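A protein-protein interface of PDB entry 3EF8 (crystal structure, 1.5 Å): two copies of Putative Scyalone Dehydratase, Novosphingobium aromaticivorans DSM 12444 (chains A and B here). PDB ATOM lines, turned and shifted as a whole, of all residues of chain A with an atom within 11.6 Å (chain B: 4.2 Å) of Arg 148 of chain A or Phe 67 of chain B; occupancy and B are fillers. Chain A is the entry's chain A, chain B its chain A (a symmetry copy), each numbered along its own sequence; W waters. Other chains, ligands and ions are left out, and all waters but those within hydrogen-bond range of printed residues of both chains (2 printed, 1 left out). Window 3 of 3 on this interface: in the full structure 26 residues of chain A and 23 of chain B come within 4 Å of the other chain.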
ATOM      1  N   TYR A 109     -23.346 -30.233 -23.922  1.00  0.00           N
ATOM      2  CA  TYR A 109     -23.077 -29.295 -25.023  1.00  0.00           C
ATOM      3  C   TYR A 109     -23.051 -27.918 -24.408  1.00  0.00           C
ATOM      4  O   TYR A 109     -24.053 -27.479 -23.858  1.00  0.00           O
ATOM      5  CB  TYR A 109     -24.136 -29.354 -26.089  1.00  0.00           C
ATOM      6  CG  TYR A 109     -24.412 -30.717 -26.641  1.00  0.00           C
ATOM      7  CD1 TYR A 109     -23.708 -31.234 -27.719  1.00  0.00           C
ATOM      8  CD2 TYR A 109     -25.401 -31.500 -26.051  1.00  0.00           C
ATOM      9  CE1 TYR A 109     -23.991 -32.498 -28.231  1.00  0.00           C
ATOM     10  CE2 TYR A 109     -25.720 -32.735 -26.576  1.00  0.00           C
ATOM     11  CZ  TYR A 109     -25.001 -33.234 -27.652  1.00  0.00           C
ATOM     12  OH  TYR A 109     -25.320 -34.477 -28.173  1.00  0.00           O
ATOM     13  N   GLN A 111     -20.984 -23.813 -23.647  1.00  0.00           N
ATOM     14  CA  GLN A 111     -20.159 -22.654 -23.980  1.00  0.00           C
ATOM     15  C   GLN A 111     -19.403 -22.244 -22.748  1.00  0.00           C
ATOM     16  O   GLN A 111     -20.003 -22.175 -21.659  1.00  0.00           O
ATOM     17  CB  GLN A 111     -21.038 -21.483 -24.428  1.00  0.00           C
ATOM     18  CG  GLN A 111     -22.004 -21.813 -25.525  1.00  0.00           C
ATOM     19  CD  GLN A 111     -22.977 -20.651 -25.812  1.00  0.00           C
ATOM     20  OE1 GLN A 111     -23.076 -19.717 -24.994  1.00  0.00           O
ATOM     21  NE2 GLN A 111     -23.704 -20.726 -26.916  1.00  0.00           N
ATOM     22  N   PHE A 113     -17.398 -19.065 -21.050  1.00  0.00           N
ATOM     23  CA  PHE A 113     -17.064 -17.648 -21.050  1.00  0.00           C
ATOM     24  C   PHE A 113     -16.019 -17.484 -19.962  1.00  0.00           C
ATOM     25  O   PHE A 113     -16.332 -17.545 -18.779  1.00  0.00           O
ATOM     26  CB  PHE A 113     -18.291 -16.768 -20.846  1.00  0.00           C
ATOM     27  CG  PHE A 113     -19.148 -16.663 -22.064  1.00  0.00           C
ATOM     28  CD1 PHE A 113     -19.966 -17.707 -22.441  1.00  0.00           C
ATOM     29  CD2 PHE A 113     -19.075 -15.562 -22.886  1.00  0.00           C
ATOM     30  CE1 PHE A 113     -20.695 -17.638 -23.611  1.00  0.00           C
ATOM     31  CE2 PHE A 113     -19.842 -15.509 -24.037  1.00  0.00           C
ATOM     32  CZ  PHE A 113     -20.648 -16.539 -24.374  1.00  0.00           C
ATOM     33  N   GLU A 129     -17.134 -19.306 -16.669  1.00  0.00           N
ATOM     34  CA  GLU A 129     -18.558 -19.389 -16.585  1.00  0.00           C
ATOM     35  C   GLU A 129     -19.025 -20.360 -17.659  1.00  0.00           C
ATOM     36  O   GLU A 129     -18.827 -20.135 -18.851  1.00  0.00           O
ATOM     37  CB  GLU A 129     -19.212 -18.038 -16.780  1.00  0.00           C
ATOM     38  CG  GLU A 129     -20.704 -18.094 -16.831  1.00  0.00           C
ATOM     39  CD  GLU A 129     -21.332 -16.734 -16.965  1.00  0.00           C
ATOM     40  OE1 GLU A 129     -20.969 -15.819 -16.188  1.00  0.00           O
ATOM     41  OE2 GLU A 129     -22.218 -16.598 -17.796  1.00  0.00           O
ATOM     42  N   ARG A 131     -21.960 -22.001 -19.698  1.00  0.00           N
ATOM     43  CA  ARG A 131     -23.348 -21.840 -20.117  1.00  0.00           C
ATOM     44  C   ARG A 131     -23.725 -23.126 -20.843  1.00  0.00           C
ATOM     45  O   ARG A 131     -22.999 -23.604 -21.687  1.00  0.00           O
ATOM     46  CB  ARG A 131     -23.552 -20.605 -20.989  1.00  0.00           C
ATOM     47  CG  ARG A 131     -23.158 -19.333 -20.262  1.00  0.00           C
ATOM     48  CD  ARG A 131     -23.438 -18.102 -21.097  1.00  0.00           C
ATOM     49  NE  ARG A 131     -22.909 -16.928 -20.428  1.00  0.00           N
ATOM     50  CZ  ARG A 131     -22.766 -15.735 -20.993  1.00  0.00           C
ATOM     51  NH1 ARG A 131     -23.141 -15.534 -22.252  1.00  0.00           N
ATOM     52  NH2 ARG A 131     -22.254 -14.747 -20.289  1.00  0.00           N
ATOM     53  N   THR A 132     -24.836 -23.745 -20.449  1.00  0.00           N
ATOM     54  CA  THR A 132     -25.235 -25.038 -20.929  1.00  0.00           C
ATOM     55  C   THR A 132     -26.244 -24.898 -22.051  1.00  0.00           C
ATOM     56  O   THR A 132     -27.364 -24.433 -21.888  1.00  0.00           O
ATOM     57  CB  THR A 132     -25.782 -25.911 -19.760  1.00  0.00           C
ATOM     58  OG1 THR A 132     -24.734 -26.113 -18.805  1.00  0.00           O
ATOM     59  CG2 THR A 132     -26.238 -27.253 -20.248  1.00  0.00           C
ATOM     60  N   THR A 133     -25.804 -25.244 -23.245  1.00  0.00           N
ATOM     61  CA  THR A 133     -26.629 -25.199 -24.432  1.00  0.00           C
ATOM     62  C   THR A 133     -27.709 -26.236 -24.391  1.00  0.00           C
ATOM     63  O   THR A 133     -28.864 -25.966 -24.699  1.00  0.00           O
ATOM     64  CB  THR A 133     -25.732 -25.409 -25.680  1.00  0.00           C
ATOM     65  OG1 THR A 133     -24.649 -24.489 -25.584  1.00  0.00           O
ATOM     66  CG2 THR A 133     -26.494 -25.227 -26.999  1.00  0.00           C
ATOM     67  N   MET A 134     -27.316 -27.432 -23.969  1.00  0.00           N
ATOM     68  CA  MET A 134     -28.230 -28.520 -23.722  1.00  0.00           C
ATOM     69  C   MET A 134     -27.443 -29.684 -23.225  1.00  0.00           C
ATOM     70  O   MET A 134     -26.214 -29.688 -23.253  1.00  0.00           O
ATOM     71  CB  MET A 134     -29.009 -28.885 -24.959  1.00  0.00           C
ATOM     72  CG  MET A 134     -28.179 -29.097 -26.141  1.00  0.00           C
ATOM     73  SD  MET A 134     -29.276 -28.685 -27.698  1.00  0.00           S
ATOM     74  CE  MET A 134     -28.512 -29.999 -28.757  1.00  0.00           C
ATOM     75  N   ALA A 143     -28.427 -25.171 -14.366  1.00  0.00           N
ATOM     76  CA  ALA A 143     -27.507 -24.666 -15.380  1.00  0.00           C
ATOM     77  C   ALA A 143     -27.669 -23.184 -15.603  1.00  0.00           C
ATOM     78  O   ALA A 143     -28.723 -22.598 -15.344  1.00  0.00           O
ATOM     79  CB  ALA A 143     -27.775 -25.386 -16.656  1.00  0.00           C
ATOM     80  N   ASN A 144     -26.591 -22.567 -16.116  1.00  0.00           N
ATOM     81  CA  ASN A 144     -26.656 -21.187 -16.608  1.00  0.00           C
ATOM     82  C   ASN A 144     -27.093 -21.272 -18.060  1.00  0.00           C
ATOM     83  O   ASN A 144     -26.483 -21.985 -18.842  1.00  0.00           O
ATOM     84  CB  ASN A 144     -25.288 -20.522 -16.599  1.00  0.00           C
ATOM     85  CG  ASN A 144     -24.720 -20.321 -15.211  1.00  0.00           C
ATOM     86  OD1 ASN A 144     -25.459 -19.913 -14.295  1.00  0.00           O
ATOM     87  ND2 ASN A 144     -23.425 -20.603 -15.027  1.00  0.00           N
ATOM     88  N   PRO A 145     -28.151 -20.577 -18.467  1.00  0.00           N
ATOM     89  CA  PRO A 145     -28.572 -20.680 -19.857  1.00  0.00           C
ATOM     90  C   PRO A 145     -27.627 -19.910 -20.769  1.00  0.00           C
ATOM     91  O   PRO A 145     -26.904 -19.042 -20.340  1.00  0.00           O
ATOM     92  CB  PRO A 145     -29.937 -20.014 -19.867  1.00  0.00           C
ATOM     93  CG  PRO A 145     -29.975 -19.170 -18.644  1.00  0.00           C
ATOM     94  CD  PRO A 145     -29.070 -19.782 -17.636  1.00  0.00           C
ATOM     95  N   ILE A 146     -27.643 -20.278 -22.056  1.00  0.00           N
ATOM     96  CA  ILE A 146     -26.836 -19.526 -23.024  1.00  0.00           C
ATOM     97  C   ILE A 146     -27.430 -18.179 -23.372  1.00  0.00           C
ATOM     98  O   ILE A 146     -26.747 -17.288 -23.829  1.00  0.00           O
ATOM     99  CB  ILE A 146     -26.520 -20.321 -24.290  1.00  0.00           C
ATOM    100  CG1 ILE A 146     -27.756 -20.658 -25.100  1.00  0.00           C
ATOM    101  CG2 ILE A 146     -25.722 -21.592 -23.922  1.00  0.00           C
ATOM    102  CD1 ILE A 146     -27.465 -21.163 -26.523  1.00  0.00           C
ATOM    103  N   GLY A 147     -28.731 -18.037 -23.134  1.00  0.00           N
ATOM    104  CA  GLY A 147     -29.426 -16.790 -23.457  1.00  0.00           C
ATOM    105  C   GLY A 147     -29.966 -16.767 -24.884  1.00  0.00           C
ATOM    106  O   GLY A 147     -30.032 -15.702 -25.516  1.00  0.00           O
ATOM    107  N   ARG A 148     -30.353 -17.924 -25.380  1.00  0.00           N
ATOM    108  CA  ARG A 148     -30.890 -18.073 -26.746  1.00  0.00           C
ATOM    109  C   ARG A 148     -32.124 -17.189 -26.947  1.00  0.00           C
ATOM    110  O   ARG A 148     -33.027 -17.199 -26.112  1.00  0.00           O
ATOM    111  CB  ARG A 148     -31.251 -19.518 -27.032  1.00  0.00           C
ATOM    112  CG  ARG A 148     -31.651 -19.821 -28.469  1.00  0.00           C
ATOM    113  CD  ARG A 148     -31.791 -21.304 -28.673  1.00  0.00           C
ATOM    114  NE  ARG A 148     -31.931 -21.698 -30.040  1.00  0.00           N
ATOM    115  CZ  ARG A 148     -33.065 -22.000 -30.651  1.00  0.00           C
ATOM    116  NH1 ARG A 148     -34.217 -21.862 -30.007  1.00  0.00           N
ATOM    117  NH2 ARG A 148     -33.059 -22.422 -31.888  1.00  0.00           N
ATOM    118  N   ALA A 149     -32.174 -16.470 -28.053  1.00  0.00           N
ATOM    119  CA  ALA A 149     -33.321 -15.579 -28.348  1.00  0.00           C
ATOM    120  C   ALA A 149     -34.517 -16.443 -28.642  1.00  0.00           C
ATOM    121  O   ALA A 149     -34.415 -17.484 -29.243  1.00  0.00           O
ATOM    122  CB  ALA A 149     -33.002 -14.654 -29.519  1.00  0.00           C
ATOM    123  N   GLU A 150     -35.677 -15.981 -28.172  1.00  0.00           N
ATOM    124  CA  GLU A 150     -36.937 -16.696 -28.366  1.00  0.00           C
ATOM    125  C   GLU A 150     -37.678 -16.067 -29.546  1.00  0.00           C
ATOM    126  O   GLU A 150     -37.067 -15.745 -30.576  1.00  0.00           O
ATOM    127  CB  GLU A 150     -37.802 -16.643 -27.093  1.00  0.00           C
ATOM    128  N   ASP B  25     -26.523 -20.707 -32.847  1.00  0.00           N
ATOM    129  CA  ASP B  25     -26.974 -21.408 -31.654  1.00  0.00           C
ATOM    130  C   ASP B  25     -27.774 -20.473 -30.742  1.00  0.00           C
ATOM    131  O   ASP B  25     -28.648 -20.912 -29.972  1.00  0.00           O
ATOM    132  CB  ASP B  25     -25.808 -21.988 -30.905  1.00  0.00           C
ATOM    133  CG  ASP B  25     -25.170 -23.205 -31.608  1.00  0.00           C
ATOM    134  OD1 ASP B  25     -25.793 -23.775 -32.526  1.00  0.00           O
ATOM    135  OD2 ASP B  25     -23.992 -23.527 -31.283  1.00  0.00           O
ATOM    136  N   MET B  26     -27.528 -19.174 -30.859  1.00  0.00           N
ATOM    137  CA  MET B  26     -28.241 -18.142 -30.057  1.00  0.00           C
ATOM    138  C   MET B  26     -29.531 -17.672 -30.727  1.00  0.00           C
ATOM    139  O   MET B  26     -30.272 -16.881 -30.150  1.00  0.00           O
ATOM    140  CB  MET B  26     -27.368 -16.950 -29.825  1.00  0.00           C
ATOM    141  CG  MET B  26     -26.169 -17.240 -28.995  1.00  0.00           C
ATOM    142  SD  MET B  26     -26.669 -17.524 -27.097  1.00  0.00           S
ATOM    143  CE  MET B  26     -27.103 -15.659 -26.726  1.00  0.00           C
ATOM    144  N   ASN B  27     -29.827 -18.151 -31.913  1.00  0.00           N
ATOM    145  CA  ASN B  27     -30.997 -17.687 -32.704  1.00  0.00           C
ATOM    146  C   ASN B  27     -30.948 -16.171 -32.972  1.00  0.00           C
ATOM    147  O   ASN B  27     -31.896 -15.425 -32.616  1.00  0.00           O
ATOM    148  CB  ASN B  27     -32.301 -18.082 -32.022  1.00  0.00           C
ATOM    149  CG  ASN B  27     -33.497 -17.808 -32.887  1.00  0.00           C
ATOM    150  OD1 ASN B  27     -33.353 -17.679 -34.089  1.00  0.00           O
ATOM    151  ND2 ASN B  27     -34.663 -17.676 -32.270  1.00  0.00           N
ATOM    152  N   ILE B  63     -35.792 -21.047 -37.127  1.00  0.00           N
ATOM    153  CA  ILE B  63     -34.713 -21.539 -36.230  1.00  0.00           C
ATOM    154  C   ILE B  63     -35.230 -21.555 -34.800  1.00  0.00           C
ATOM    155  O   ILE B  63     -35.005 -22.492 -34.059  1.00  0.00           O
ATOM    156  CB  ILE B  63     -33.430 -20.660 -36.276  1.00  0.00           C
ATOM    157  CG1 ILE B  63     -32.708 -20.810 -37.606  1.00  0.00           C
ATOM    158  CG2 ILE B  63     -32.420 -21.038 -35.139  1.00  0.00           C
ATOM    159  CD1 ILE B  63     -31.521 -19.907 -37.724  1.00  0.00           C
ATOM    160  N   GLY B  64     -35.986 -20.525 -34.447  1.00  0.00           N
ATOM    161  CA  GLY B  64     -36.425 -20.319 -33.085  1.00  0.00           C
ATOM    162  C   GLY B  64     -37.634 -21.149 -32.727  1.00  0.00           C
ATOM    163  O   GLY B  64     -37.918 -21.385 -31.550  1.00  0.00           O
ATOM    164  N   THR B  65     -38.320 -21.616 -33.751  1.00  0.00           N
ATOM    165  CA  THR B  65     -39.613 -22.275 -33.571  1.00  0.00           C
ATOM    166  C   THR B  65     -39.529 -23.785 -33.727  1.00  0.00           C
ATOM    167  O   THR B  65     -40.193 -24.548 -33.014  1.00  0.00           O
ATOM    168  CB  THR B  65     -40.659 -21.712 -34.570  1.00  0.00           C
ATOM    169  OG1 THR B  65     -40.134 -21.763 -35.899  1.00  0.00           O
ATOM    170  CG2 THR B  65     -41.006 -20.269 -34.212  1.00  0.00           C
ATOM    171  N   PHE B  66     -38.698 -24.237 -34.655  1.00  0.00           N
ATOM    172  CA  PHE B  66     -38.574 -25.674 -34.929  1.00  0.00           C
ATOM    173  C   PHE B  66     -37.530 -26.366 -34.042  1.00  0.00           C
ATOM    174  O   PHE B  66     -37.526 -27.590 -33.923  1.00  0.00           O
ATOM    175  CB  PHE B  66     -38.263 -25.917 -36.406  1.00  0.00           C
ATOM    176  CG  PHE B  66     -39.439 -25.656 -37.318  1.00  0.00           C
ATOM    177  N   PHE B  67     -36.658 -25.572 -33.431  1.00  0.00           N
ATOM    178  CA  PHE B  67     -35.645 -26.109 -32.511  1.00  0.00           C
ATOM    179  C   PHE B  67     -35.713 -25.414 -31.172  1.00  0.00           C
ATOM    180  O   PHE B  67     -35.904 -24.189 -31.095  1.00  0.00           O
ATOM    181  CB  PHE B  67     -34.194 -25.891 -33.011  1.00  0.00           C
ATOM    182  CG  PHE B  67     -33.941 -26.296 -34.429  1.00  0.00           C
ATOM    183  CD1 PHE B  67     -33.980 -27.622 -34.831  1.00  0.00           C
ATOM    184  CD2 PHE B  67     -33.606 -25.336 -35.366  1.00  0.00           C
ATOM    185  CE1 PHE B  67     -33.750 -27.983 -36.150  1.00  0.00           C
ATOM    186  CE2 PHE B  67     -33.358 -25.695 -36.690  1.00  0.00           C
ATOM    187  CZ  PHE B  67     -33.436 -27.023 -37.075  1.00  0.00           C
ATOM    188  N   ARG B  68     -35.545 -26.188 -30.117  1.00  0.00           N
ATOM    189  CA  ARG B  68     -35.399 -25.634 -28.771  1.00  0.00           C
ATOM    190  C   ARG B  68     -33.951 -25.232 -28.545  1.00  0.00           C
ATOM    191  O   ARG B  68     -33.649 -24.420 -27.679  1.00  0.00           O
ATOM    192  CB  ARG B  68     -35.822 -26.641 -27.708  1.00  0.00           C
ATOM    193  CG  ARG B  68     -37.302 -26.972 -27.771  1.00  0.00           C
ATOM    194  CD  ARG B  68     -37.674 -27.903 -26.651  1.00  0.00           C
ATOM    195  NE  ARG B  68     -37.257 -29.266 -26.925  1.00  0.00           N
ATOM    196  CZ  ARG B  68     -37.155 -30.205 -25.996  1.00  0.00           C
ATOM    197  NH1 ARG B  68     -37.430 -29.916 -24.734  1.00  0.00           N
ATOM    198  NH2 ARG B  68     -36.797 -31.436 -26.320  1.00  0.00           N
ATOM    199  N   GLY B  69     -33.059 -25.842 -29.322  1.00  0.00           N
ATOM    200  CA  GLY B  69     -31.637 -25.523 -29.218  1.00  0.00           C
ATOM    201  C   GLY B  69     -30.842 -26.250 -30.266  1.00  0.00           C
ATOM    202  O   GLY B  69     -31.282 -27.263 -30.781  1.00  0.00           O
ATOM    203  N   THR B  70     -29.679 -25.673 -30.565  1.00  0.00           N
ATOM    204  CA  THR B  70     -28.677 -26.302 -31.434  1.00  0.00           C
ATOM    205  C   THR B  70     -27.297 -26.075 -30.824  1.00  0.00           C
ATOM    206  O   THR B  70     -27.063 -25.136 -30.059  1.00  0.00           O
ATOM    207  CB  THR B  70     -28.696 -25.750 -32.887  1.00  0.00           C
ATOM    208  OG1 THR B  70     -28.412 -24.365 -32.902  1.00  0.00           O
ATOM    209  CG2 THR B  70     -30.026 -25.903 -33.584  1.00  0.00           C
ATOM    210  N   HIS B  97     -29.120 -30.908 -33.047  1.00  0.00           N
ATOM    211  CA  HIS B  97     -30.390 -30.194 -33.047  1.00  0.00           C
ATOM    212  C   HIS B  97     -31.421 -30.823 -32.116  1.00  0.00           C
ATOM    213  O   HIS B  97     -31.743 -32.008 -32.274  1.00  0.00           O
ATOM    214  CB  HIS B  97     -30.961 -30.225 -34.472  1.00  0.00           C
ATOM    215  CG  HIS B  97     -30.034 -29.705 -35.515  1.00  0.00           C
ATOM    216  ND1 HIS B  97     -28.971 -30.457 -35.966  1.00  0.00           N
ATOM    217  CD2 HIS B  97     -30.012 -28.549 -36.210  1.00  0.00           C
ATOM    218  CE1 HIS B  97     -28.305 -29.755 -36.866  1.00  0.00           C
ATOM    219  NE2 HIS B  97     -28.926 -28.610 -37.050  1.00  0.00           N
ATOM    220  N   ARG B  98     -31.902 -30.014 -31.177  1.00  0.00           N
ATOM    221  CA  ARG B  98     -32.941 -30.475 -30.205  1.00  0.00           C
ATOM    222  C   ARG B  98     -34.228 -29.830 -30.710  1.00  0.00           C
ATOM    223  O   ARG B  98     -34.375 -28.605 -30.770  1.00  0.00           O
ATOM    224  CB  ARG B  98     -32.639 -30.037 -28.781  1.00  0.00           C
ATOM    225  CG  ARG B  98     -33.758 -30.520 -27.845  1.00  0.00           C
ATOM    226  CD  ARG B  98     -33.315 -30.902 -26.500  1.00  0.00           C
ATOM    227  NE  ARG B  98     -32.351 -31.975 -26.545  1.00  0.00           N
ATOM    228  CZ  ARG B  98     -31.585 -32.296 -25.517  1.00  0.00           C
ATOM    229  NH1 ARG B  98     -31.682 -31.606 -24.398  1.00  0.00           N
ATOM    230  NH2 ARG B  98     -30.687 -33.241 -25.654  1.00  0.00           N
ATOM    231  N   TYR B  99     -35.129 -30.713 -31.141  1.00  0.00           N
ATOM    232  CA  TYR B  99     -36.341 -30.266 -31.791  1.00  0.00           C
ATOM    233  C   TYR B  99     -37.412 -29.804 -30.811  1.00  0.00           C
ATOM    234  O   TYR B  99     -37.440 -30.218 -29.689  1.00  0.00           O
ATOM    235  CB  TYR B  99     -36.886 -31.384 -32.687  1.00  0.00           C
ATOM    236  CG  TYR B  99     -35.920 -31.769 -33.786  1.00  0.00           C
ATOM    237  CD1 TYR B  99     -35.842 -31.018 -34.952  1.00  0.00           C
ATOM    238  CD2 TYR B  99     -35.112 -32.896 -33.657  1.00  0.00           C
ATOM    239  CE1 TYR B  99     -34.928 -31.353 -35.976  1.00  0.00           C
ATOM    240  CE2 TYR B  99     -34.227 -33.252 -34.675  1.00  0.00           C
ATOM    241  CZ  TYR B  99     -34.148 -32.483 -35.809  1.00  0.00           C
ATOM    242  OH  TYR B  99     -33.235 -32.859 -36.782  1.00  0.00           O
ATOM    243  N   THR B 100     -38.288 -28.944 -31.316  1.00  0.00           N
ATOM    244  CA  THR B 100     -39.445 -28.468 -30.543  1.00  0.00           C
ATOM    245  C   THR B 100     -40.524 -29.553 -30.503  1.00  0.00           C
ATOM    246  O   THR B 100     -41.236 -29.682 -29.511  1.00  0.00           O
ATOM    247  CB  THR B 100     -39.959 -27.133 -31.082  1.00  0.00           C
ATOM    248  OG1 THR B 100     -40.125 -27.207 -32.500  1.00  0.00           O
ATOM    249  CG2 THR B 100     -38.967 -26.038 -30.742  1.00  0.00           C
ATOM    250  N   HIS B 139     -33.624 -34.131 -39.885  1.00  0.00           N
ATOM    251  CA  HIS B 139     -34.899 -33.597 -40.473  1.00  0.00           C
ATOM    252  C   HIS B 139     -34.765 -33.180 -41.907  1.00  0.00           C
ATOM    253  O   HIS B 139     -35.675 -32.641 -42.520  1.00  0.00           O
ATOM    254  CB  HIS B 139     -35.427 -32.442 -39.652  1.00  0.00           C
ATOM    255  CG  HIS B 139     -34.531 -31.259 -39.677  1.00  0.00           C
ATOM    256  ND1 HIS B 139     -33.326 -31.240 -39.008  1.00  0.00           N
ATOM    257  CD2 HIS B 139     -34.642 -30.069 -40.302  1.00  0.00           C
ATOM    258  CE1 HIS B 139     -32.732 -30.079 -39.230  1.00  0.00           C
ATOM    259  NE2 HIS B 139     -33.510 -29.353 -40.015  1.00  0.00           N
HETATM  260  O   HOH W   1     -23.109 -22.912 -28.688  1.00  0.00           O
HETATM  261  O   HOH W   2     -30.211 -22.374 -32.529  1.00  0.00           O
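The backbone carbonyl oxygen (O) of Tyr 109 of chain A sits at hydrogen-bond distance from the backbone NH (N) of Thr 133 of chain A, 2.9 Å away. O of Met 134 of chain A lies within hydrogen-bond range of N of Tyr 109 of chain A (3.0 Å). The side-chain carboxylate (OD1) of Asp 25 of chain B is in hydrogen-bond range of the side-chain hydroxyl (OG1) of Thr 70 of chain B (2.7 Å). The backbone NH (N) of Arg 68 of chain B is in hydrogen-bond range of the backbone carbonyl oxygen (O) of Arg 98 of chain B (2.8 Å). O of Tyr 99 of chain B sits at hydrogen-bond distance from NE of Arg 68 of chain B. The backbone carbonyl oxygen (O) of Gly 69 of chain B sits at hydrogen-bond distance from the backbone NH (N) of Arg 98 of chain B (2.8 Å).
Water W2 lies within hydrogen-bond range of the side-chain hydroxyl (OG1) of Thr 70 of chain B (2.7 Å), the guanidinium group (NH2) of Arg 148 of chain A (2.9 Å) and the backbone carbonyl oxygen (O) of Asp 25 of chain B (3.3 Å). Water W1 lies within hydrogen-bond range of OD2 of Asp 25 of chain B (2.8 Å) and NE2 of Gln 111 of chain A (2.9 Å).
No position is printed for both chains. Of the 15 pairs that touch across the chains among the printed residues, none has its exchanged pair printed and touching as well.
Hydrophobic or aromatic side chains of chain A within 4 Å of the printed part of chain B: Met 134, Ile 146 and Ala 149. Of the 16 printed residues of chain B, 9 touch a printed residue of chain A. Hydrophobic or aromatic side chains of chain B within 4 Å of the printed part of chain A: Met 26, Ile 63 and Phe 67. Among the printed residues, no Asp or Glu carboxylate lies within 4 Å of a Lys or Arg side-chain nitrogen of the other chain.
Printed residues of chain B within 4 Å of Arg 148 of chain A: Asp 25, Met 26, Ile 63, Phe 67, Arg 68 and Gly 69. Phe 67 of chain B touches just one residue of chain A: Arg 148 (3.1 Å). Met 26 of chain B touches just these residues of chain A: Ile 146 (3.3 Å), Gly 147 (3.2 Å), Arg 148 (3.7 Å) and Ala 149 (2.9 Å). Ile 63 of chain B touches one residue of chain A. No residue of chain A comes within 4 Å of Gly 64 of chain B. No residue of chain A comes within 4 Å of Thr 65 of chain B. No residue of chain A comes within 4 Å of Tyr 99 of chain B. Printed residues of chain A within 4 Å of Thr 70 of chain B: Thr 133 (3.1 Å). Of the printed residues of chain A, Asp 25 of chain B touches Ile 146 (3.7 Å) and Arg 148 (3.4 Å). Of the printed residues of chain B, Thr 133 of chain A touches Thr 70 (3.1 Å). Ala 143 of chain A touches none of the printed residues of chain B. Pro 145 of chain A touches none of the printed residues of chain B.
O of Asp 25 of chain B sits at hydrogen-bond distance from NE of Arg 148 of chain A (3.4 Å). The guanidinium group (NH2) of Arg 148 of chain A lies within hydrogen-bond range of the backbone carbonyl oxygen (O) of Ile 63 of chain B. The guanidinium group (NH1) of Arg 148 of chain A sits at hydrogen-bond distance from the backbone carbonyl oxygen (O) of Phe 67 of chain B (3.1 Å). N of Ala 149 of chain A is in hydrogen-bond range of O of Met 26 of chain B. The backbone carbonyl oxygen of Ala 149 of chain A sits at hydrogen-bond distance from the side-chain amide nitrogen of Asn 27 of chain B (3.0 Å). The side-chain sulfur (SD) of Met 26 of chain B sits close to the backbone carbonyl oxygen (O) of Ile 146 of chain A.
Thr 133 of chain A touches Thr 70 of chain B (CG2 to O, 3.1 Å). C of Gly 69 of chain B touches SD of Met 134 of chain A, 3.9 Å away. Arg 98 of chain B touches Met 134 of chain A. Asp 25 of chain B touches Ile 146 of chain A. Met 26 of chain B touches Gly 147 of chain A (CE to O, 3.2 Å). Arg 148 of chain A touches Met 26 of chain B. O of Arg 68 of chain B touches NH1 of Arg 148 of chain A (3.5 Å). Gly 69 of chain B touches Arg 148 of chain A (CA to NE, 3.9 Å). Glu 150 of chain A touches Asn 27 of chain B (O to ND2, 3.5 Å).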
